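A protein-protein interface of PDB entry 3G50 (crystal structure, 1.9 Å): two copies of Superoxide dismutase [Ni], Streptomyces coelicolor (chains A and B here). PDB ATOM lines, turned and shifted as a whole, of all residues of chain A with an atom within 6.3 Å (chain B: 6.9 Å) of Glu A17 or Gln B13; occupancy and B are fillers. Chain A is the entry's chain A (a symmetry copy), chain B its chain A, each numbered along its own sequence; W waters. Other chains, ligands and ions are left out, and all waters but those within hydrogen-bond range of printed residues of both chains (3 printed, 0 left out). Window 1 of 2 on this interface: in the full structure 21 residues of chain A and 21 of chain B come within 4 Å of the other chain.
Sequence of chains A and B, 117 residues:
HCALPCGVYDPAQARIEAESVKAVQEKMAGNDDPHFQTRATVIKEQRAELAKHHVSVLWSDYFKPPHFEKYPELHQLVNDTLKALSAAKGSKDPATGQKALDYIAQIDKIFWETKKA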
ATOM      1  N   ALA A  12      -5.711   3.745 -24.123  1.00  0.00           N
ATOM      2  CA  ALA A  12      -5.852   2.738 -25.180  1.00  0.00           C
ATOM      3  C   ALA A  12      -6.508   1.447 -24.663  1.00  0.00           C
ATOM      4  O   ALA A  12      -7.189   0.788 -25.427  1.00  0.00           O
ATOM      5  CB  ALA A  12      -4.488   2.385 -25.830  1.00  0.00           C
ATOM      6  N   GLN A  13      -6.248   1.054 -23.416  1.00  0.00           N
ATOM      7  CA  GLN A  13      -6.866  -0.186 -22.881  1.00  0.00           C
ATOM      8  C   GLN A  13      -8.409  -0.035 -22.806  1.00  0.00           C
ATOM      9  O   GLN A  13      -9.167  -0.915 -23.258  1.00  0.00           O
ATOM     10  CB  GLN A  13      -6.300  -0.550 -21.492  1.00  0.00           C
ATOM     11  CG  GLN A  13      -4.734  -0.741 -21.429  1.00  0.00           C
ATOM     12  CD  GLN A  13      -4.277  -1.325 -20.067  1.00  0.00           C
ATOM     13  OE1 GLN A  13      -4.262  -0.629 -19.037  1.00  0.00           O
ATOM     14  NE2 GLN A  13      -3.888  -2.594 -20.078  1.00  0.00           N
ATOM     15  N   ALA A  14      -8.875   1.072 -22.230  1.00  0.00           N
ATOM     16  CA  ALA A  14     -10.312   1.331 -22.192  1.00  0.00           C
ATOM     17  C   ALA A  14     -10.867   1.422 -23.610  1.00  0.00           C
ATOM     18  O   ALA A  14     -11.918   0.814 -23.899  1.00  0.00           O
ATOM     19  CB  ALA A  14     -10.639   2.604 -21.420  1.00  0.00           C
ATOM     20  N   ARG A  15     -10.202   2.203 -24.467  1.00  0.00           N
ATOM     21  CA  ARG A  15     -10.665   2.370 -25.851  1.00  0.00           C
ATOM     22  C   ARG A  15     -10.797   1.049 -26.612  1.00  0.00           C
ATOM     23  O   ARG A  15     -11.790   0.831 -27.262  1.00  0.00           O
ATOM     24  CB  ARG A  15      -9.793   3.354 -26.656  1.00  0.00           C
ATOM     25  CG  ARG A  15     -10.174   3.369 -28.169  1.00  0.00           C
ATOM     26  CD  ARG A  15      -9.174   4.126 -29.038  1.00  0.00           C
ATOM     27  NE  ARG A  15      -7.792   3.684 -28.794  1.00  0.00           N
ATOM     28  CZ  ARG A  15      -7.185   2.674 -29.417  1.00  0.00           C
ATOM     29  NH1 ARG A  15      -7.812   1.959 -30.335  1.00  0.00           N
ATOM     30  NH2 ARG A  15      -5.936   2.368 -29.105  1.00  0.00           N
ATOM     31  N   ILE A  16      -9.772   0.181 -26.571  1.00  0.00           N
ATOM     32  CA  ILE A  16      -9.847  -1.104 -27.276  1.00  0.00           C
ATOM     33  C   ILE A  16     -11.062  -1.917 -26.825  1.00  0.00           C
ATOM     34  O   ILE A  16     -11.766  -2.509 -27.672  1.00  0.00           O
ATOM     35  CB  ILE A  16      -8.487  -1.928 -27.147  1.00  0.00           C
ATOM     36  CG1 ILE A  16      -7.354  -1.157 -27.878  1.00  0.00           C
ATOM     37  CG2 ILE A  16      -8.535  -3.285 -27.884  1.00  0.00           C
ATOM     38  CD1 ILE A  16      -5.848  -1.541 -27.502  1.00  0.00           C
ATOM     39  N   GLU A  17     -11.306  -1.970 -25.507  1.00  0.00           N
ATOM     40  CA  GLU A  17     -12.427  -2.766 -24.991  1.00  0.00           C
ATOM     41  C   GLU A  17     -13.778  -2.111 -25.425  1.00  0.00           C
ATOM     42  O   GLU A  17     -14.745  -2.813 -25.806  1.00  0.00           O
ATOM     43  CB  GLU A  17     -12.311  -2.954 -23.459  1.00  0.00           C
ATOM     44  CG  GLU A  17     -11.052  -3.814 -23.050  1.00  0.00           C
ATOM     45  CD  GLU A  17     -11.062  -5.231 -23.603  1.00  0.00           C
ATOM     46  OE1 GLU A  17      -9.987  -5.879 -23.650  1.00  0.00           O
ATOM     47  OE2 GLU A  17     -12.155  -5.738 -23.971  1.00  0.00           O
ATOM     48  N   ALA A  18     -13.816  -0.781 -25.419  1.00  0.00           N
ATOM     49  CA  ALA A  18     -15.058  -0.068 -25.851  1.00  0.00           C
ATOM     50  C   ALA A  18     -15.263  -0.167 -27.375  1.00  0.00           C
ATOM     51  O   ALA A  18     -16.398  -0.127 -27.857  1.00  0.00           O
ATOM     52  CB  ALA A  18     -14.981   1.345 -25.443  1.00  0.00           C
ATOM     53  N   GLU A  19     -14.167  -0.272 -28.126  1.00  0.00           N
ATOM     54  CA  GLU A  19     -14.238  -0.567 -29.566  1.00  0.00           C
ATOM     55  C   GLU A  19     -14.855  -1.930 -29.790  1.00  0.00           C
ATOM     56  O   GLU A  19     -15.698  -2.094 -30.710  1.00  0.00           O
ATOM     57  CB  GLU A  19     -12.855  -0.456 -30.277  1.00  0.00           C
ATOM     58  CG  GLU A  19     -12.513   0.995 -30.629  1.00  0.00           C
ATOM     59  CD  GLU A  19     -11.089   1.230 -31.128  1.00  0.00           C
ATOM     60  OE1 GLU A  19     -10.736   2.424 -31.269  1.00  0.00           O
ATOM     61  OE2 GLU A  19     -10.324   0.263 -31.376  1.00  0.00           O
ATOM     62  N   SER A  20     -14.455  -2.906 -28.958  1.00  0.00           N
ATOM     63  CA  SER A  20     -15.037  -4.226 -29.058  1.00  0.00           C
ATOM     64  C   SER A  20     -16.551  -4.204 -28.800  1.00  0.00           C
ATOM     65  O   SER A  20     -17.309  -4.876 -29.495  1.00  0.00           O
ATOM     66  CB  SER A  20     -14.323  -5.205 -28.119  1.00  0.00           C
ATOM     67  OG  SER A  20     -12.959  -5.258 -28.527  1.00  0.00           O
ATOM     68  N   VAL A  21     -16.976  -3.447 -27.791  1.00  0.00           N
ATOM     69  CA  VAL A  21     -18.402  -3.313 -27.494  1.00  0.00           C
ATOM     70  C   VAL A  21     -19.132  -2.858 -28.781  1.00  0.00           C
ATOM     71  O   VAL A  21     -20.166  -3.441 -29.165  1.00  0.00           O
ATOM     72  CB  VAL A  21     -18.614  -2.347 -26.364  1.00  0.00           C
ATOM     73  CG1 VAL A  21     -20.148  -1.921 -26.171  1.00  0.00           C
ATOM     74  CG2 VAL A  21     -18.039  -2.970 -25.049  1.00  0.00           C
ATOM     75  N   LYS A  22     -18.603  -1.822 -29.414  1.00  0.00           N
ATOM     76  CA  LYS A  22     -19.316  -1.252 -30.595  1.00  0.00           C
ATOM     77  C   LYS A  22     -19.295  -2.246 -31.744  1.00  0.00           C
ATOM     78  O   LYS A  22     -20.285  -2.425 -32.438  1.00  0.00           O
ATOM     79  CB  LYS A  22     -18.751   0.107 -31.001  1.00  0.00           C
ATOM     80  CG  LYS A  22     -19.626   0.826 -32.087  1.00  0.00           C
ATOM     81  CD  LYS A  22     -18.950   2.110 -32.642  1.00  0.00           C
ATOM     82  CE  LYS A  22     -19.757   2.614 -33.887  1.00  0.00           C
ATOM     83  NZ  LYS A  22     -19.460   3.965 -34.442  1.00  0.00           N
ATOM     84  N   GLN A  46     -19.029  -8.573 -21.044  1.00  0.00           N
ATOM     85  CA  GLN A  46     -17.687  -8.745 -20.496  1.00  0.00           C
ATOM     86  C   GLN A  46     -16.800  -7.600 -20.929  1.00  0.00           C
ATOM     87  O   GLN A  46     -16.115  -6.977 -20.088  1.00  0.00           O
ATOM     88  CB  GLN A  46     -17.071 -10.073 -20.982  1.00  0.00           C
ATOM     89  CG  GLN A  46     -17.723 -11.265 -20.426  1.00  0.00           C
ATOM     90  CD  GLN A  46     -17.332 -12.614 -21.108  1.00  0.00           C
ATOM     91  OE1 GLN A  46     -16.873 -12.663 -22.277  1.00  0.00           O
ATOM     92  NE2 GLN A  46     -17.554 -13.700 -20.388  1.00  0.00           N
ATOM     93  N   ARG A  47     -16.785  -7.305 -22.225  1.00  0.00           N
ATOM     94  CA  ARG A  47     -15.903  -6.248 -22.742  1.00  0.00           C
ATOM     95  C   ARG A  47     -16.283  -4.882 -22.162  1.00  0.00           C
ATOM     96  O   ARG A  47     -15.424  -4.039 -21.885  1.00  0.00           O
ATOM     97  CB  ARG A  47     -15.950  -6.199 -24.285  1.00  0.00           C
ATOM     98  CG  ARG A  47     -15.532  -7.481 -24.991  1.00  0.00           C
ATOM     99  CD  ARG A  47     -14.079  -7.715 -24.736  1.00  0.00           C
ATOM    100  NE  ARG A  47     -13.755  -9.105 -24.542  1.00  0.00           N
ATOM    101  CZ  ARG A  47     -12.546  -9.558 -24.212  1.00  0.00           C
ATOM    102  NH1 ARG A  47     -11.517  -8.717 -24.039  1.00  0.00           N
ATOM    103  NH2 ARG A  47     -12.360 -10.866 -24.080  1.00  0.00           N
ATOM    104  N   ALA A  48     -17.573  -4.644 -22.010  1.00  0.00           N
ATOM    105  CA  ALA A  48     -18.028  -3.353 -21.457  1.00  0.00           C
ATOM    106  C   ALA A  48     -17.567  -3.221 -20.012  1.00  0.00           C
ATOM    107  O   ALA A  48     -17.141  -2.154 -19.591  1.00  0.00           O
ATOM    108  CB  ALA A  48     -19.551  -3.224 -21.555  1.00  0.00           C
ATOM    109  N   LEU A  50     -14.860  -4.636 -18.681  1.00  0.00           N
ATOM    110  CA  LEU A  50     -13.418  -4.387 -18.661  1.00  0.00           C
ATOM    111  C   LEU A  50     -13.103  -2.915 -19.026  1.00  0.00           C
ATOM    112  O   LEU A  50     -12.226  -2.257 -18.432  1.00  0.00           O
ATOM    113  CB  LEU A  50     -12.710  -5.275 -19.650  1.00  0.00           C
ATOM    114  CG  LEU A  50     -12.449  -6.729 -19.356  1.00  0.00           C
ATOM    115  CD1 LEU A  50     -11.986  -7.366 -20.665  1.00  0.00           C
ATOM    116  CD2 LEU A  50     -11.342  -6.837 -18.249  1.00  0.00           C
ATOM    117  N   ALA A  51     -13.829  -2.412 -20.012  1.00  0.00           N
ATOM    118  CA  ALA A  51     -13.697  -0.997 -20.371  1.00  0.00           C
ATOM    119  C   ALA A  51     -13.944  -0.134 -19.147  1.00  0.00           C
ATOM    120  O   ALA A  51     -13.146   0.771 -18.886  1.00  0.00           O
ATOM    121  CB  ALA A  51     -14.625  -0.638 -21.463  1.00  0.00           C
ATOM    122  N   LYS A  52     -14.987  -0.438 -18.366  1.00  0.00           N
ATOM    123  CA  LYS A  52     -15.320   0.379 -17.202  1.00  0.00           C
ATOM    124  C   LYS A  52     -14.183   0.278 -16.169  1.00  0.00           C
ATOM    125  O   LYS A  52     -13.782   1.267 -15.526  1.00  0.00           O
ATOM    126  CB  LYS A  52     -16.657  -0.053 -16.587  1.00  0.00           C
ATOM    127  CG  LYS A  52     -17.873   0.538 -17.314  1.00  0.00           C
ATOM    128  CD  LYS A  52     -19.189  -0.176 -16.939  1.00  0.00           C
ATOM    129  CE  LYS A  52     -19.572   0.100 -15.493  1.00  0.00           C
ATOM    130  NZ  LYS A  52     -20.843  -0.647 -15.055  1.00  0.00           N
ATOM    131  N   HIS A  54     -10.950  -0.268 -16.800  1.00  0.00           N
ATOM    132  CA  HIS A  54      -9.805   0.536 -17.279  1.00  0.00           C
ATOM    133  C   HIS A  54     -10.011   2.020 -17.020  1.00  0.00           C
ATOM    134  O   HIS A  54      -9.080   2.721 -16.641  1.00  0.00           O
ATOM    135  CB  HIS A  54      -9.527   0.307 -18.770  1.00  0.00           C
ATOM    136  CG  HIS A  54      -8.977  -1.048 -19.064  1.00  0.00           C
ATOM    137  ND1 HIS A  54      -8.000  -1.619 -18.286  1.00  0.00           N
ATOM    138  CD2 HIS A  54      -9.312  -1.978 -20.000  1.00  0.00           C
ATOM    139  CE1 HIS A  54      -7.728  -2.833 -18.740  1.00  0.00           C
ATOM    140  NE2 HIS A  54      -8.502  -3.070 -19.786  1.00  0.00           N
ATOM    141  N   LEU A  85     -20.719   3.588 -20.839  1.00  0.00           N
ATOM    142  CA  LEU A  85     -20.358   2.187 -21.017  1.00  0.00           C
ATOM    143  C   LEU A  85     -21.460   1.261 -20.446  1.00  0.00           C
ATOM    144  O   LEU A  85     -21.768   0.244 -21.052  1.00  0.00           O
ATOM    145  CB  LEU A  85     -19.010   1.921 -20.328  1.00  0.00           C
ATOM    146  CG  LEU A  85     -17.806   2.536 -21.047  1.00  0.00           C
ATOM    147  CD1 LEU A  85     -16.556   2.452 -20.139  1.00  0.00           C
ATOM    148  CD2 LEU A  85     -17.603   1.816 -22.364  1.00  0.00           C
ATOM    149  N   HIS B   1     -10.749  -9.801 -30.006  1.00  0.00           N
ATOM    150  CA  HIS B   1      -9.998 -10.469 -28.901  1.00  0.00           C
ATOM    151  C   HIS B   1     -10.915 -11.332 -28.009  1.00  0.00           C
ATOM    152  O   HIS B   1     -10.590 -11.624 -26.852  1.00  0.00           O
ATOM    153  CB  HIS B   1      -9.201  -9.431 -28.094  1.00  0.00           C
ATOM    154  CG  HIS B   1      -9.986  -8.209 -27.725  1.00  0.00           C
ATOM    155  ND1 HIS B   1     -11.179  -8.268 -27.029  1.00  0.00           N
ATOM    156  CD2 HIS B   1      -9.739  -6.896 -27.935  1.00  0.00           C
ATOM    157  CE1 HIS B   1     -11.629  -7.044 -26.830  1.00  0.00           C
ATOM    158  NE2 HIS B   1     -10.778  -6.192 -27.376  1.00  0.00           N
ATOM    159  N   VAL B   8     -11.830  -6.961 -33.410  1.00  0.00           N
ATOM    160  CA  VAL B   8     -11.021  -5.878 -32.767  1.00  0.00           C
ATOM    161  C   VAL B   8      -9.764  -6.438 -32.039  1.00  0.00           C
ATOM    162  O   VAL B   8      -9.821  -6.890 -30.897  1.00  0.00           O
ATOM    163  CB  VAL B   8     -11.838  -4.978 -31.795  1.00  0.00           C
ATOM    164  CG1 VAL B   8     -10.933  -3.911 -31.127  1.00  0.00           C
ATOM    165  CG2 VAL B   8     -12.995  -4.291 -32.512  1.00  0.00           C
ATOM    166  N   TYR B   9      -8.636  -6.411 -32.731  1.00  0.00           N
ATOM    167  CA  TYR B   9      -7.381  -6.884 -32.186  1.00  0.00           C
ATOM    168  C   TYR B   9      -6.387  -5.756 -32.251  1.00  0.00           C
ATOM    169  O   TYR B   9      -6.461  -4.904 -33.139  1.00  0.00           O
ATOM    170  CB  TYR B   9      -6.883  -8.126 -32.947  1.00  0.00           C
ATOM    171  CG  TYR B   9      -7.801  -9.306 -32.724  1.00  0.00           C
ATOM    172  CD1 TYR B   9      -8.843  -9.597 -33.631  1.00  0.00           C
ATOM    173  CD2 TYR B   9      -7.693 -10.081 -31.567  1.00  0.00           C
ATOM    174  CE1 TYR B   9      -9.722 -10.649 -33.401  1.00  0.00           C
ATOM    175  CE2 TYR B   9      -8.568 -11.144 -31.331  1.00  0.00           C
ATOM    176  CZ  TYR B   9      -9.572 -11.420 -32.241  1.00  0.00           C
ATOM    177  OH  TYR B   9     -10.414 -12.474 -31.976  1.00  0.00           O
ATOM    178  N   ASP B  10      -5.468  -5.742 -31.294  1.00  0.00           N
ATOM    179  CA  ASP B  10      -4.373  -4.793 -31.307  1.00  0.00           C
ATOM    180  C   ASP B  10      -3.298  -5.242 -30.318  1.00  0.00           C
ATOM    181  O   ASP B  10      -3.577  -5.368 -29.121  1.00  0.00           O
ATOM    182  CB  ASP B  10      -4.884  -3.411 -30.934  1.00  0.00           C
ATOM    183  CG  ASP B  10      -3.821  -2.329 -31.049  1.00  0.00           C
ATOM    184  OD1 ASP B  10      -2.614  -2.638 -31.268  1.00  0.00           O
ATOM    185  OD2 ASP B  10      -4.221  -1.148 -30.939  1.00  0.00           O
ATOM    186  N   PRO B  11      -2.067  -5.481 -30.816  1.00  0.00           N
ATOM    187  CA  PRO B  11      -0.949  -5.902 -29.977  1.00  0.00           C
ATOM    188  C   PRO B  11      -0.608  -4.871 -28.903  1.00  0.00           C
ATOM    189  O   PRO B  11       0.118  -5.197 -27.966  1.00  0.00           O
ATOM    190  CB  PRO B  11       0.210  -6.058 -30.984  1.00  0.00           C
ATOM    191  CG  PRO B  11      -0.451  -6.280 -32.259  1.00  0.00           C
ATOM    192  CD  PRO B  11      -1.636  -5.333 -32.210  1.00  0.00           C
ATOM    193  N   ALA B  12      -1.156  -3.655 -29.005  1.00  0.00           N
ATOM    194  CA  ALA B  12      -1.032  -2.679 -27.917  1.00  0.00           C
ATOM    195  C   ALA B  12      -1.432  -3.276 -26.558  1.00  0.00           C
ATOM    196  O   ALA B  12      -0.888  -2.860 -25.552  1.00  0.00           O
ATOM    197  CB  ALA B  12      -1.883  -1.408 -28.180  1.00  0.00           C
ATOM    198  N   GLN B  13      -2.415  -4.175 -26.520  1.00  0.00           N
ATOM    199  CA  GLN B  13      -2.827  -4.775 -25.225  1.00  0.00           C
ATOM    200  C   GLN B  13      -1.666  -5.611 -24.621  1.00  0.00           C
ATOM    201  O   GLN B  13      -1.324  -5.474 -23.431  1.00  0.00           O
ATOM    202  CB  GLN B  13      -4.087  -5.653 -25.381  1.00  0.00           C
ATOM    203  CG  GLN B  13      -5.350  -4.921 -25.982  1.00  0.00           C
ATOM    204  CD  GLN B  13      -6.625  -5.799 -25.890  1.00  0.00           C
ATOM    205  OE1 GLN B  13      -6.796  -6.773 -26.644  1.00  0.00           O
ATOM    206  NE2 GLN B  13      -7.520  -5.435 -24.981  1.00  0.00           N
ATOM    207  N   ALA B  14      -1.067  -6.479 -25.434  1.00  0.00           N
ATOM    208  CA  ALA B  14       0.087  -7.245 -24.969  1.00  0.00           C
ATOM    209  C   ALA B  14       1.220  -6.302 -24.579  1.00  0.00           C
ATOM    210  O   ALA B  14       1.830  -6.484 -23.504  1.00  0.00           O
ATOM    211  CB  ALA B  14       0.571  -8.236 -26.019  1.00  0.00           C
ATOM    212  N   ARG B  15       1.530  -5.340 -25.454  1.00  0.00           N
ATOM    213  CA  ARG B  15       2.617  -4.391 -25.178  1.00  0.00           C
ATOM    214  C   ARG B  15       2.438  -3.624 -23.866  1.00  0.00           C
ATOM    215  O   ARG B  15       3.368  -3.517 -23.106  1.00  0.00           O
ATOM    216  CB  ARG B  15       2.850  -3.400 -26.336  1.00  0.00           C
ATOM    217  CG  ARG B  15       3.865  -2.279 -25.952  1.00  0.00           C
ATOM    218  CD  ARG B  15       3.925  -1.141 -26.966  1.00  0.00           C
ATOM    219  NE  ARG B  15       2.587  -0.622 -27.287  1.00  0.00           N
ATOM    220  CZ  ARG B  15       1.955   0.343 -26.620  1.00  0.00           C
ATOM    221  NH1 ARG B  15       2.507   0.925 -25.569  1.00  0.00           N
ATOM    222  NH2 ARG B  15       0.746   0.721 -27.002  1.00  0.00           N
ATOM    223  N   ILE B  16       1.250  -3.048 -23.617  1.00  0.00           N
ATOM    224  CA  ILE B  16       1.021  -2.307 -22.371  1.00  0.00           C
ATOM    225  C   ILE B  16       1.291  -3.181 -21.145  1.00  0.00           C
ATOM    226  O   ILE B  16       1.926  -2.715 -20.175  1.00  0.00           O
ATOM    227  CB  ILE B  16      -0.432  -1.650 -22.334  1.00  0.00           C
ATOM    228  CG1 ILE B  16      -0.528  -0.568 -23.444  1.00  0.00           C
ATOM    229  CG2 ILE B  16      -0.701  -0.860 -21.034  1.00  0.00           C
ATOM    230  CD1 ILE B  16      -1.994  -0.111 -23.894  1.00  0.00           C
ATOM    231  N   GLU B  17       0.807  -4.433 -21.168  1.00  0.00           N
ATOM    232  CA  GLU B  17       0.987  -5.319 -20.011  1.00  0.00           C
ATOM    233  C   GLU B  17       2.498  -5.687 -19.863  1.00  0.00           C
ATOM    234  O   GLU B  17       3.045  -5.736 -18.735  1.00  0.00           O
ATOM    235  CB  GLU B  17       0.070  -6.562 -20.121  1.00  0.00           C
ATOM    236  CG  GLU B  17      -1.462  -6.191 -20.044  1.00  0.00           C
ATOM    237  CD  GLU B  17      -1.876  -5.533 -18.737  1.00  0.00           C
ATOM    238  OE1 GLU B  17      -2.951  -4.885 -18.691  1.00  0.00           O
ATOM    239  OE2 GLU B  17      -1.149  -5.680 -17.719  1.00  0.00           O
ATOM    240  N   ALA B  18       3.170  -5.884 -20.994  1.00  0.00           N
ATOM    241  CA  ALA B  18       4.630  -6.209 -20.950  1.00  0.00           C
ATOM    242  C   ALA B  18       5.466  -4.977 -20.549  1.00  0.00           C
ATOM    243  O   ALA B  18       6.546  -5.118 -19.967  1.00  0.00           O
ATOM    244  CB  ALA B  18       5.064  -6.707 -22.265  1.00  0.00           C
ATOM    245  N   LEU B  50      -1.200 -11.710 -18.111  1.00  0.00           N
ATOM    246  CA  LEU B  50      -2.138 -11.059 -19.026  1.00  0.00           C
ATOM    247  C   LEU B  50      -1.475 -10.783 -20.399  1.00  0.00           C
ATOM    248  O   LEU B  50      -2.081 -10.956 -21.475  1.00  0.00           O
ATOM    249  CB  LEU B  50      -2.608  -9.744 -18.462  1.00  0.00           C
ATOM    250  CG  LEU B  50      -3.647  -9.681 -17.373  1.00  0.00           C
ATOM    251  CD1 LEU B  50      -3.661  -8.242 -16.861  1.00  0.00           C
ATOM    252  CD2 LEU B  50      -5.041 -10.085 -17.971  1.00  0.00           C
ATOM    253  N   ALA B  51      -0.226 -10.349 -20.343  1.00  0.00           N
ATOM    254  CA  ALA B  51       0.539 -10.160 -21.579  1.00  0.00           C
ATOM    255  C   ALA B  51       0.547 -11.451 -22.377  1.00  0.00           C
ATOM    256  O   ALA B  51       0.280 -11.406 -23.582  1.00  0.00           O
ATOM    257  CB  ALA B  51       1.916  -9.714 -21.286  1.00  0.00           C
ATOM    258  N   HIS B  54      -2.832 -12.005 -24.040  1.00  0.00           N
ATOM    259  CA  HIS B  54      -3.044 -11.138 -25.221  1.00  0.00           C
ATOM    260  C   HIS B  54      -2.297 -11.658 -26.440  1.00  0.00           C
ATOM    261  O   HIS B  54      -2.817 -11.624 -27.549  1.00  0.00           O
ATOM    262  CB  HIS B  54      -2.637  -9.686 -24.947  1.00  0.00           C
ATOM    263  CG  HIS B  54      -3.554  -8.988 -24.000  1.00  0.00           C
ATOM    264  ND1 HIS B  54      -4.919  -9.110 -24.089  1.00  0.00           N
ATOM    265  CD2 HIS B  54      -3.310  -8.221 -22.902  1.00  0.00           C
ATOM    266  CE1 HIS B  54      -5.487  -8.427 -23.108  1.00  0.00           C
ATOM    267  NE2 HIS B  54      -4.534  -7.869 -22.381  1.00  0.00           N
ATOM    268  N   VAL B  55      -1.078 -12.143 -26.236  1.00  0.00           N
ATOM    269  CA  VAL B  55      -0.280 -12.674 -27.351  1.00  0.00           C
ATOM    270  C   VAL B  55      -0.914 -13.938 -27.926  1.00  0.00           C
ATOM    271  O   VAL B  55      -1.115 -14.079 -29.162  1.00  0.00           O
ATOM    272  CB  VAL B  55       1.169 -12.964 -26.898  1.00  0.00           C
ATOM    273  CG1 VAL B  55       1.912 -13.802 -27.909  1.00  0.00           C
ATOM    274  CG2 VAL B  55       1.914 -11.641 -26.593  1.00  0.00           C
ATOM    275  N   VAL B  57      -4.009 -14.874 -27.745  1.00  0.00           N
ATOM    276  CA  VAL B  57      -5.236 -14.504 -28.446  1.00  0.00           C
ATOM    277  C   VAL B  57      -4.981 -14.011 -29.875  1.00  0.00           C
ATOM    278  O   VAL B  57      -5.730 -14.368 -30.795  1.00  0.00           O
ATOM    279  CB  VAL B  57      -6.032 -13.481 -27.611  1.00  0.00           C
ATOM    280  CG1 VAL B  57      -7.097 -12.782 -28.472  1.00  0.00           C
ATOM    281  CG2 VAL B  57      -6.725 -14.247 -26.482  1.00  0.00           C
ATOM    282  N   LEU B  58      -3.952 -13.183 -30.055  1.00  0.00           N
ATOM    283  CA  LEU B  58      -3.623 -12.692 -31.404  1.00  0.00           C
ATOM    284  C   LEU B  58      -3.278 -13.881 -32.303  1.00  0.00           C
ATOM    285  O   LEU B  58      -3.679 -13.957 -33.476  1.00  0.00           O
ATOM    286  CB  LEU B  58      -2.435 -11.727 -31.379  1.00  0.00           C
ATOM    287  CG  LEU B  58      -2.571 -10.320 -30.796  1.00  0.00           C
ATOM    288  CD1 LEU B  58      -1.194  -9.609 -30.767  1.00  0.00           C
ATOM    289  CD2 LEU B  58      -3.642  -9.433 -31.496  1.00  0.00           C
HETATM  290  O   HOH W   1      -6.816  -0.236 -32.237  1.00  0.00           O
HETATM  291  O   HOH W   2      -4.602  -5.978 -20.300  1.00  0.00           O
HETATM  292  O   HOH W   3      -8.538  -5.148 -21.680  1.00  0.00           O
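Gln A13 touches Ile B16, and with the chains exchanged Ile A16 touches Gln B13.
Gln A13 touches Glu B17, and with the chains exchanged Glu A17 touches Gln B13.
Of the 12 pairs that touch across the chains among the printed residues, 4 have their exchanged pair printed and touching as well.
Glu A17 touches just these residues of chain B: His B1 and Gln B13.
Gln B13 touches two residues of chain A.
Of the printed residues of chain B, Arg A47 touches His B1.
Of the printed residues of chain A, Val B8 touches Ile A16, Glu A19 and Ser A20.
The nearest residue of chain B that does not touch Glu A17 is His B54 (5.2 Å).
Water W3 lies within hydrogen-bond range of OE1 of Glu A17 (2.6 Å), NE2 of His A54 (2.8 Å) and NE2 of Gln B13 (3.5 Å).
Water W2 lies within hydrogen-bond range of OE1 of Glu B17, NE2 of His B54 and NE2 of Gln A13.
Water W1 lies within hydrogen-bond range of the side-chain carboxylate (OD2) of Asp B10 and the guanidinium group (NH1) of Arg A15.
A ring nitrogen (NE2) of His B1 lies within hydrogen-bond range of the side-chain hydroxyl of Ser A20, 2.6 Å away.
A ring nitrogen (ND1) of His B1 sits at hydrogen-bond distance from the guanidinium group (NH1) of Arg A47, at 3.0 Å.
The side-chain carboxylate (OE1) of Glu A17 sits at hydrogen-bond distance from the side-chain amide nitrogen (NE2) of Gln B13.
OE1 of Glu B17 lies within hydrogen-bond range of NE2 of Gln A13 (2.8 Å).
CG2 of Ile B16 touches CD of Gln A13 (3.7 Å).
Ile A16 touches His B1 (CG2 to NE2, 3.7 Å).
Ile A16 touches Val B8.
OD2 of Asp B10 touches CD1 of Ile A16, at 3.8 Å.
CG2 of Ile A16 touches CD of Gln B13, at 3.7 Å.
Glu A17 touches His B1 (OE2 to CE1, 3.2 Å).
O of Glu A19 touches CG2 of Val B8, at 3.9 Å.
Ser A20 touches Val B8 (OG to CB, 3.5 Å).
Of the 19 printed residues of chain A, 6 touch a printed residue of chain B.
Hydrophobic or aromatic side chains of chain A that line the printed part of chain B: Ile A16.
Printed residues of chain B that touch a printed residue of chain A: His B1, Val B8, Asp B10, Gln B13, Ile B16 and Glu B17.
Among the printed residues, no Asp or Glu carboxylate lies within 4 Å of a Lys or Arg side-chain nitrogen of the other chain.
O of Val B8 sits close to N of His B1.
The backbone NH of His B1 lies close to the side-chain hydroxyl of Tyr B9, 3.3 Å away.
OD1 of Asp B10 is in hydrogen-bond range of N of Ala B12.
The guanidinium group of Arg A15 is in salt-bridge range of the side-chain carboxylate of Glu A19.
The side-chain hydroxyl (OG) of Ser A20 sits at hydrogen-bond distance from the backbone carbonyl oxygen (O) of Ile A16, at 3.1 Å.
The guanidinium group of Arg A47 is in salt-bridge range of the side-chain carboxylate of Glu A17 (3.0 Å).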
